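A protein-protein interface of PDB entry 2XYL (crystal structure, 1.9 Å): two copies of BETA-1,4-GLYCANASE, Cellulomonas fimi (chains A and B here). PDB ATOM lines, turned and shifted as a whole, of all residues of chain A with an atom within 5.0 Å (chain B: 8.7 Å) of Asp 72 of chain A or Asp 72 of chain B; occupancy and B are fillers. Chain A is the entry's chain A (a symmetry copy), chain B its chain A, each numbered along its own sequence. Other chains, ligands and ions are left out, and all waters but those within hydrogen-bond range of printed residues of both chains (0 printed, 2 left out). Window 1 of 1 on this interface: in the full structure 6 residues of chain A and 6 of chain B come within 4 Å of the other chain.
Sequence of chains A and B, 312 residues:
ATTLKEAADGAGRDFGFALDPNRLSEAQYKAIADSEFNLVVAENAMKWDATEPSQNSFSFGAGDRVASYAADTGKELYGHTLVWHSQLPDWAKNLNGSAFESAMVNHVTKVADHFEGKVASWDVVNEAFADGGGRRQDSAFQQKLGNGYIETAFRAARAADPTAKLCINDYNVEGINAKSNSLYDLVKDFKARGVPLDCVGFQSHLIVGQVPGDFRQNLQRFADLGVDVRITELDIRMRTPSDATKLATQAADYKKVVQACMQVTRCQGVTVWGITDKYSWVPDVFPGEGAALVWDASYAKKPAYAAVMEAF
The backbone carbonyl oxygen of Asp 72 of chain A sits at hydrogen-bond distance from the side-chain amino group of Lys 30 of chain B (3.4 Å). The guanidinium group (NH2) of Arg 65 of chain B lies within salt-bridge range of the side-chain carboxylate (OD1) of Asp 72 of chain A, 2.9 Å away. NZ of Lys 30 of chain A is in hydrogen-bond range of O of Asp 72 of chain B (3.4 Å). NH2 of Arg 65 of chain A is in salt-bridge range of OD1 of Asp 72 of chain B, at 2.9 Å. The side-chain carboxylate of Asp 72 of chain B sits close to the side-chain carboxylate of Asp 72 of chain A (2.7 Å).
Lys 30 of chain A touches Ala 71 of chain B, and with the chains exchanged Ala 71 of chain A touches Lys 30 of chain B. Arg 65 of chain A touches Asp 72 of chain B, and with the chains exchanged Asp 72 of chain A touches Arg 65 of chain B. Ser 68 of chain A touches its own counterpart, Ser 68 of chain B. Asp 72 of chain B touches its own counterpart, Asp 72 of chain A.
Of the printed residues of chain B, Arg 65 of chain A touches Ser 68 (3.2 Å), Ala 71 (3.7 Å) and Asp 72 (2.9 Å). Of chain B, only Lys 30 and Arg 65 come within 4 Å of Ala 71 of chain A. Asp 72 of chain A touches just these residues of chain B: Lys 30 (3.4 Å), Arg 65 (2.9 Å), Ser 68 (3.7 Å), Tyr 69 (3.3 Å) and Asp 72 (2.7 Å). No residue of chain B comes within 4 Å of Thr 73 of chain A. Of the printed residues of chain A, Lys 30 of chain B touches Ala 71 (3.5 Å) and Asp 72 (3.4 Å). Of the printed residues of chain A, Arg 65 of chain B touches Ser 68 (3.2 Å), Ala 71 (3.7 Å) and Asp 72 (2.9 Å). Of the printed residues of chain A, Ser 68 of chain B touches Arg 65 (3.2 Å), Ser 68 (3.5 Å) and Asp 72 (3.7 Å). Of the printed residues of chain A, Tyr 69 of chain B touches Asp 72 (3.3 Å). Of the printed residues of chain A, Asp 72 of chain B touches Lys 30, Arg 65, Ser 68, Tyr 69 and Asp 72.
Printed residues of chain A that touch a printed residue of chain B: Lys 30, Arg 65, Ser 68, Tyr 69, Ala 71 and Asp 72. Of the 19 printed residues of chain B, 6 touch a printed residue of chain A. Hydrophobic or aromatic side chains of chain B that line the printed part of chain A: Tyr 69 and Ala 71. Among the printed residues, 16 pairs touch across the chains.
OD2 of Asp 34 of chain B is in salt-bridge range of NZ of Lys 30 of chain B (2.7 Å). The side-chain hydroxyl (OH) of Tyr 69 of chain B sits at hydrogen-bond distance from the side-chain carboxylate (OD1) of Asp 34 of chain B (2.8 Å). O of Asp 64 of chain B sits at hydrogen-bond distance from OG of Ser 68 of chain B (3.1 Å). OG1 of Thr 73 of chain B lies within hydrogen-bond range of O of Tyr 69 of chain B (2.6 Å). The backbone carbonyl oxygen (O) of Tyr 69 of chain A sits at hydrogen-bond distance from the side-chain hydroxyl (OG1) of Thr 73 of chain A, 2.6 Å away.
Among the printed residues, pairs that only touch across the chains: Arg 65 of chain A with Ser 68 of chain B, Ser 68 of chain A with Arg 65 of chain B, Asp 72 of chain A with Tyr 69 of chain B, Tyr 69 of chain A with Asp 72 of chain B, Ser 68 of chain A with Ser 68 of chain B, Lys 30 of chain A with Ala 71 of chain B, Ala 71 of chain A with Lys 30 of chain B, Asp 72 of chain A with Ser 68 of chain B, Ser 68 of chain A with Asp 72 of chain B, Arg 65 of chain A with Ala 71 of chain B and Ala 71 of chain A with Arg 65 of chain B.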
ATOM      1  N   LEU A  24      11.166  18.514  -9.342  1.00  0.00           N
ATOM      2  CA  LEU A  24      11.956  17.717  -8.407  1.00  0.00           C
ATOM      3  C   LEU A  24      13.212  18.447  -7.925  1.00  0.00           C
ATOM      4  O   LEU A  24      13.843  18.032  -6.953  1.00  0.00           O
ATOM      5  CB  LEU A  24      12.334  16.367  -9.025  1.00  0.00           C
ATOM      6  CG  LEU A  24      11.186  15.386  -9.261  1.00  0.00           C
ATOM      7  CD1 LEU A  24      11.699  14.176 -10.029  1.00  0.00           C
ATOM      8  CD2 LEU A  24      10.556  14.971  -7.934  1.00  0.00           C
ATOM      9  N   LYS A  30       9.902  18.045  -3.757  1.00  0.00           N
ATOM     10  CA  LYS A  30      10.459  16.697  -3.693  1.00  0.00           C
ATOM     11  C   LYS A  30      10.221  16.038  -2.341  1.00  0.00           C
ATOM     12  O   LYS A  30       9.911  14.854  -2.272  1.00  0.00           O
ATOM     13  CB  LYS A  30      11.959  16.731  -3.982  1.00  0.00           C
ATOM     14  CG  LYS A  30      12.597  15.359  -4.086  1.00  0.00           C
ATOM     15  CD  LYS A  30      14.112  15.457  -4.022  1.00  0.00           C
ATOM     16  CE  LYS A  30      14.771  14.153  -4.444  1.00  0.00           C
ATOM     17  NZ  LYS A  30      14.240  12.972  -3.706  1.00  0.00           N
ATOM     18  N   ARG A  65      12.221  10.043 -17.054  1.00  0.00           N
ATOM     19  CA  ARG A  65      12.544  10.721 -15.801  1.00  0.00           C
ATOM     20  C   ARG A  65      11.501  10.420 -14.730  1.00  0.00           C
ATOM     21  O   ARG A  65      11.841  10.231 -13.562  1.00  0.00           O
ATOM     22  CB  ARG A  65      12.681  12.230 -16.017  1.00  0.00           C
ATOM     23  CG  ARG A  65      13.148  12.986 -14.784  1.00  0.00           C
ATOM     24  CD  ARG A  65      14.560  12.577 -14.391  1.00  0.00           C
ATOM     25  NE  ARG A  65      14.987  13.152 -13.116  1.00  0.00           N
ATOM     26  CZ  ARG A  65      14.810  12.566 -11.934  1.00  0.00           C
ATOM     27  NH1 ARG A  65      14.205  11.385 -11.853  1.00  0.00           N
ATOM     28  NH2 ARG A  65      15.264  13.145 -10.830  1.00  0.00           N
ATOM     29  N   SER A  68      11.919   6.712 -13.753  1.00  0.00           N
ATOM     30  CA  SER A  68      13.102   6.549 -12.910  1.00  0.00           C
ATOM     31  C   SER A  68      12.771   6.948 -11.479  1.00  0.00           C
ATOM     32  O   SER A  68      13.122   6.244 -10.536  1.00  0.00           O
ATOM     33  CB  SER A  68      14.263   7.404 -13.423  1.00  0.00           C
ATOM     34  OG  SER A  68      14.776   6.906 -14.642  1.00  0.00           O
ATOM     35  N   TYR A  69      12.070   8.069 -11.331  1.00  0.00           N
ATOM     36  CA  TYR A  69      11.677   8.569 -10.018  1.00  0.00           C
ATOM     37  C   TYR A  69      10.844   7.548  -9.249  1.00  0.00           C
ATOM     38  O   TYR A  69      11.077   7.320  -8.065  1.00  0.00           O
ATOM     39  CB  TYR A  69      10.901   9.883 -10.145  1.00  0.00           C
ATOM     40  CG  TYR A  69      10.357  10.378  -8.824  1.00  0.00           C
ATOM     41  CD1 TYR A  69      11.196  10.974  -7.886  1.00  0.00           C
ATOM     42  CD2 TYR A  69       9.015  10.198  -8.489  1.00  0.00           C
ATOM     43  CE1 TYR A  69      10.712  11.373  -6.647  1.00  0.00           C
ATOM     44  CE2 TYR A  69       8.525  10.593  -7.254  1.00  0.00           C
ATOM     45  CZ  TYR A  69       9.378  11.175  -6.338  1.00  0.00           C
ATOM     46  OH  TYR A  69       8.902  11.544  -5.103  1.00  0.00           O
ATOM     47  N   ALA A  70       9.878   6.939  -9.932  1.00  0.00           N
ATOM     48  CA  ALA A  70       9.014   5.939  -9.313  1.00  0.00           C
ATOM     49  C   ALA A  70       9.834   4.745  -8.836  1.00  0.00           C
ATOM     50  O   ALA A  70       9.688   4.300  -7.701  1.00  0.00           O
ATOM     51  CB  ALA A  70       7.955   5.483 -10.300  1.00  0.00           C
ATOM     52  N   ALA A  71      10.708   4.251  -9.709  1.00  0.00           N
ATOM     53  CA  ALA A  71      11.559   3.108  -9.401  1.00  0.00           C
ATOM     54  C   ALA A  71      12.544   3.393  -8.267  1.00  0.00           C
ATOM     55  O   ALA A  71      12.770   2.540  -7.409  1.00  0.00           O
ATOM     56  CB  ALA A  71      12.312   2.662 -10.651  1.00  0.00           C
ATOM     57  N   ASP A  72      13.107   4.597  -8.262  1.00  0.00           N
ATOM     58  CA  ASP A  72      14.077   5.007  -7.249  1.00  0.00           C
ATOM     59  C   ASP A  72      13.482   5.289  -5.875  1.00  0.00           C
ATOM     60  O   ASP A  72      14.181   5.189  -4.862  1.00  0.00           O
ATOM     61  CB  ASP A  72      14.864   6.229  -7.730  1.00  0.00           C
ATOM     62  CG  ASP A  72      15.708   5.940  -8.962  1.00  0.00           C
ATOM     63  OD1 ASP A  72      16.116   4.777  -9.166  1.00  0.00           O
ATOM     64  OD2 ASP A  72      15.967   6.884  -9.733  1.00  0.00           O
ATOM     65  N   THR A  73      12.200   5.647  -5.838  1.00  0.00           N
ATOM     66  CA  THR A  73      11.525   5.946  -4.579  1.00  0.00           C
ATOM     67  C   THR A  73      10.557   4.851  -4.120  1.00  0.00           C
ATOM     68  O   THR A  73       9.960   4.944  -3.044  1.00  0.00           O
ATOM     69  CB  THR A  73      10.797   7.305  -4.638  1.00  0.00           C
ATOM     70  OG1 THR A  73       9.913   7.333  -5.765  1.00  0.00           O
ATOM     71  CG2 THR A  73      11.804   8.436  -4.756  1.00  0.00           C
ATOM     72  N   GLY A  74      10.417   3.809  -4.939  1.00  0.00           N
ATOM     73  CA  GLY A  74       9.549   2.695  -4.607  1.00  0.00           C
ATOM     74  C   GLY A  74       8.058   2.931  -4.757  1.00  0.00           C
ATOM     75  O   GLY A  74       7.263   2.342  -4.021  1.00  0.00           O
ATOM     76  N   LEU B  19      28.090   2.361 -10.824  1.00  0.00           N
ATOM     77  CA  LEU B  19      26.740   1.869 -11.040  1.00  0.00           C
ATOM     78  C   LEU B  19      26.435   1.276 -12.404  1.00  0.00           C
ATOM     79  O   LEU B  19      26.821   1.815 -13.440  1.00  0.00           O
ATOM     80  CB  LEU B  19      25.728   2.986 -10.763  1.00  0.00           C
ATOM     81  CG  LEU B  19      24.247   2.673 -11.018  1.00  0.00           C
ATOM     82  CD1 LEU B  19      23.734   1.705  -9.966  1.00  0.00           C
ATOM     83  CD2 LEU B  19      23.419   3.953 -11.006  1.00  0.00           C
ATOM     84  N   PRO B  21      23.120   0.521 -14.099  1.00  0.00           N
ATOM     85  CA  PRO B  21      21.678   0.762 -13.998  1.00  0.00           C
ATOM     86  C   PRO B  21      20.786  -0.479 -14.088  1.00  0.00           C
ATOM     87  O   PRO B  21      19.740  -0.534 -13.443  1.00  0.00           O
ATOM     88  CB  PRO B  21      21.417   1.759 -15.133  1.00  0.00           C
ATOM     89  CG  PRO B  21      22.510   1.477 -16.107  1.00  0.00           C
ATOM     90  CD  PRO B  21      23.695   1.307 -15.202  1.00  0.00           C
ATOM     91  N   LEU B  24      19.745  -2.215 -10.645  1.00  0.00           N
ATOM     92  CA  LEU B  24      18.833  -1.587  -9.691  1.00  0.00           C
ATOM     93  C   LEU B  24      17.535  -2.377  -9.509  1.00  0.00           C
ATOM     94  O   LEU B  24      16.781  -2.133  -8.567  1.00  0.00           O
ATOM     95  CB  LEU B  24      18.522  -0.145 -10.104  1.00  0.00           C
ATOM     96  CG  LEU B  24      19.679   0.849 -10.015  1.00  0.00           C
ATOM     97  CD1 LEU B  24      19.254   2.181 -10.616  1.00  0.00           C
ATOM     98  CD2 LEU B  24      20.131   1.016  -8.567  1.00  0.00           C
ATOM     99  N   SER B  25      17.278  -3.316 -10.417  1.00  0.00           N
ATOM    100  CA  SER B  25      16.086  -4.154 -10.348  1.00  0.00           C
ATOM    101  C   SER B  25      16.314  -5.308  -9.370  1.00  0.00           C
ATOM    102  O   SER B  25      15.390  -6.051  -9.042  1.00  0.00           O
ATOM    103  CB  SER B  25      15.729  -4.697 -11.734  1.00  0.00           C
ATOM    104  OG  SER B  25      16.730  -5.574 -12.223  1.00  0.00           O
ATOM    105  N   LYS B  30      20.284  -2.755  -4.950  1.00  0.00           N
ATOM    106  CA  LYS B  30      19.708  -1.434  -4.720  1.00  0.00           C
ATOM    107  C   LYS B  30      19.765  -1.026  -3.254  1.00  0.00           C
ATOM    108  O   LYS B  30      20.050   0.124  -2.937  1.00  0.00           O
ATOM    109  CB  LYS B  30      18.257  -1.399  -5.198  1.00  0.00           C
ATOM    110  CG  LYS B  30      17.623  -0.023  -5.139  1.00  0.00           C
ATOM    111  CD  LYS B  30      16.113  -0.113  -5.285  1.00  0.00           C
ATOM    112  CE  LYS B  30      15.498   1.252  -5.550  1.00  0.00           C
ATOM    113  NZ  LYS B  30      15.918   2.278  -4.555  1.00  0.00           N
ATOM    114  N   ASP B  34      21.676   2.262  -2.093  1.00  0.00           N
ATOM    115  CA  ASP B  34      20.912   3.328  -1.439  1.00  0.00           C
ATOM    116  C   ASP B  34      21.462   3.784  -0.092  1.00  0.00           C
ATOM    117  O   ASP B  34      21.483   4.977   0.192  1.00  0.00           O
ATOM    118  CB  ASP B  34      19.454   2.902  -1.209  1.00  0.00           C
ATOM    119  CG  ASP B  34      18.646   2.779  -2.495  1.00  0.00           C
ATOM    120  OD1 ASP B  34      19.018   3.367  -3.532  1.00  0.00           O
ATOM    121  OD2 ASP B  34      17.606   2.090  -2.452  1.00  0.00           O
ATOM    122  N   VAL B  40      27.858   8.554  -6.835  1.00  0.00           N
ATOM    123  CA  VAL B  40      27.659   7.519  -7.836  1.00  0.00           C
ATOM    124  C   VAL B  40      28.290   7.908  -9.177  1.00  0.00           C
ATOM    125  O   VAL B  40      28.393   9.089  -9.512  1.00  0.00           O
ATOM    126  CB  VAL B  40      26.150   7.196  -8.008  1.00  0.00           C
ATOM    127  CG1 VAL B  40      25.407   8.389  -8.563  1.00  0.00           C
ATOM    128  CG2 VAL B  40      25.956   5.980  -8.898  1.00  0.00           C
ATOM    129  N   ASP B  64      21.185   8.906 -18.565  1.00  0.00           N
ATOM    130  CA  ASP B  64      20.163   9.635 -17.822  1.00  0.00           C
ATOM    131  C   ASP B  64      19.677   8.815 -16.631  1.00  0.00           C
ATOM    132  O   ASP B  64      19.350   9.376 -15.583  1.00  0.00           O
ATOM    133  CB  ASP B  64      18.965   9.964 -18.722  1.00  0.00           C
ATOM    134  CG  ASP B  64      19.279  11.019 -19.769  1.00  0.00           C
ATOM    135  OD1 ASP B  64      20.066  11.947 -19.491  1.00  0.00           O
ATOM    136  OD2 ASP B  64      18.715  10.924 -20.881  1.00  0.00           O
ATOM    137  N   ARG B  65      19.581   7.497 -16.809  1.00  0.00           N
ATOM    138  CA  ARG B  65      19.109   6.611 -15.747  1.00  0.00           C
ATOM    139  C   ARG B  65      20.005   6.706 -14.516  1.00  0.00           C
ATOM    140  O   ARG B  65      19.517   6.690 -13.385  1.00  0.00           O
ATOM    141  CB  ARG B  65      19.018   5.166 -16.241  1.00  0.00           C
ATOM    142  CG  ARG B  65      18.407   4.209 -15.231  1.00  0.00           C
ATOM    143  CD  ARG B  65      16.952   4.559 -14.954  1.00  0.00           C
ATOM    144  NE  ARG B  65      16.373   3.772 -13.865  1.00  0.00           N
ATOM    145  CZ  ARG B  65      16.392   4.138 -12.586  1.00  0.00           C
ATOM    146  NH1 ARG B  65      16.968   5.279 -12.222  1.00  0.00           N
ATOM    147  NH2 ARG B  65      15.808   3.378 -11.668  1.00  0.00           N
ATOM    148  N   VAL B  66      21.310   6.828 -14.750  1.00  0.00           N
ATOM    149  CA  VAL B  66      22.280   6.955 -13.667  1.00  0.00           C
ATOM    150  C   VAL B  66      22.105   8.319 -13.000  1.00  0.00           C
ATOM    151  O   VAL B  66      22.086   8.417 -11.772  1.00  0.00           O
ATOM    152  CB  VAL B  66      23.733   6.818 -14.184  1.00  0.00           C
ATOM    153  CG1 VAL B  66      24.719   7.017 -13.042  1.00  0.00           C
ATOM    154  CG2 VAL B  66      23.939   5.459 -14.840  1.00  0.00           C
ATOM    155  N   ALA B  67      21.957   9.360 -13.819  1.00  0.00           N
ATOM    156  CA  ALA B  67      21.771  10.722 -13.323  1.00  0.00           C
ATOM    157  C   ALA B  67      20.486  10.849 -12.506  1.00  0.00           C
ATOM    158  O   ALA B  67      20.461  11.540 -11.487  1.00  0.00           O
ATOM    159  CB  ALA B  67      21.764  11.714 -14.485  1.00  0.00           C
ATOM    160  N   SER B  68      19.424  10.188 -12.960  1.00  0.00           N
ATOM    161  CA  SER B  68      18.142  10.213 -12.259  1.00  0.00           C
ATOM    162  C   SER B  68      18.292   9.564 -10.891  1.00  0.00           C
ATOM    163  O   SER B  68      17.816  10.094  -9.890  1.00  0.00           O
ATOM    164  CB  SER B  68      17.064   9.476 -13.058  1.00  0.00           C
ATOM    165  OG  SER B  68      16.705  10.187 -14.225  1.00  0.00           O
ATOM    166  N   TYR B  69      18.982   8.426 -10.855  1.00  0.00           N
ATOM    167  CA  TYR B  69      19.210   7.698  -9.612  1.00  0.00           C
ATOM    168  C   TYR B  69      19.927   8.557  -8.576  1.00  0.00           C
ATOM    169  O   TYR B  69      19.543   8.575  -7.409  1.00  0.00           O
ATOM    170  CB  TYR B  69      20.011   6.419  -9.870  1.00  0.00           C
ATOM    171  CG  TYR B  69      20.389   5.691  -8.599  1.00  0.00           C
ATOM    172  CD1 TYR B  69      19.445   4.949  -7.894  1.00  0.00           C
ATOM    173  CD2 TYR B  69      21.675   5.794  -8.070  1.00  0.00           C
ATOM    174  CE1 TYR B  69      19.772   4.331  -6.694  1.00  0.00           C
ATOM    175  CE2 TYR B  69      22.009   5.182  -6.872  1.00  0.00           C
ATOM    176  CZ  TYR B  69      21.054   4.456  -6.189  1.00  0.00           C
ATOM    177  OH  TYR B  69      21.373   3.870  -4.988  1.00  0.00           O
ATOM    178  N   ALA B  70      20.966   9.266  -9.011  1.00  0.00           N
ATOM    179  CA  ALA B  70      21.732  10.132  -8.121  1.00  0.00           C
ATOM    180  C   ALA B  70      20.846  11.232  -7.549  1.00  0.00           C
ATOM    181  O   ALA B  70      20.841  11.467  -6.344  1.00  0.00           O
ATOM    182  CB  ALA B  70      22.903  10.742  -8.869  1.00  0.00           C
ATOM    183  N   ALA B  71      20.084  11.882  -8.424  1.00  0.00           N
ATOM    184  CA  ALA B  71      19.187  12.963  -8.030  1.00  0.00           C
ATOM    185  C   ALA B  71      18.070  12.493  -7.098  1.00  0.00           C
ATOM    186  O   ALA B  71      17.727  13.183  -6.140  1.00  0.00           O
ATOM    187  CB  ALA B  71      18.594  13.630  -9.267  1.00  0.00           C
ATOM    188  N   ASP B  72      17.524  11.313  -7.378  1.00  0.00           N
ATOM    189  CA  ASP B  72      16.438  10.742  -6.585  1.00  0.00           C
ATOM    190  C   ASP B  72      16.858  10.214  -5.217  1.00  0.00           C
ATOM    191  O   ASP B  72      16.034  10.141  -4.300  1.00  0.00           O
ATOM    192  CB  ASP B  72      15.733   9.633  -7.370  1.00  0.00           C
ATOM    193  CG  ASP B  72      15.049  10.145  -8.628  1.00  0.00           C
ATOM    194  OD1 ASP B  72      14.657  11.330  -8.674  1.00  0.00           O
ATOM    195  OD2 ASP B  72      14.901   9.355  -9.581  1.00  0.00           O
ATOM    196  N   THR B  73      18.128   9.841  -5.082  1.00  0.00           N
ATOM    197  CA  THR B  73      18.642   9.316  -3.820  1.00  0.00           C
ATOM    198  C   THR B  73      19.531  10.303  -3.057  1.00  0.00           C
ATOM    199  O   THR B  73      19.987  10.013  -1.947  1.00  0.00           O
ATOM    200  CB  THR B  73      19.387   7.981  -4.025  1.00  0.00           C
ATOM    201  OG1 THR B  73      20.406   8.143  -5.019  1.00  0.00           O
ATOM    202  CG2 THR B  73      18.415   6.900  -4.469  1.00  0.00           C
ATOM    203  N   GLY B  74      19.761  11.471  -3.654  1.00  0.00           N
ATOM    204  CA  GLY B  74      20.568  12.498  -3.023  1.00  0.00           C
ATOM    205  C   GLY B  74      22.069  12.276  -3.022  1.00  0.00           C
ATOM    206  O   GLY B  74      22.757  12.717  -2.098  1.00  0.00           O
ATOM    207  N   LYS B  75      22.578  11.597  -4.046  1.00  0.00           N
ATOM    208  CA  LYS B  75      24.008  11.329  -4.155  1.00  0.00           C
ATOM    209  C   LYS B  75      24.635  12.254  -5.188  1.00  0.00           C
ATOM    210  O   LYS B  75      23.960  12.713  -6.116  1.00  0.00           O
ATOM    211  CB  LYS B  75      24.254   9.884  -4.596  1.00  0.00           C
ATOM    212  CG  LYS B  75      23.578   8.831  -3.744  1.00  0.00           C
ATOM    213  CD  LYS B  75      23.899   7.434  -4.247  1.00  0.00           C
ATOM    214  CE  LYS B  75      23.000   6.403  -3.591  1.00  0.00           C
ATOM    215  NZ  LYS B  75      23.090   6.421  -2.105  1.00  0.00           N
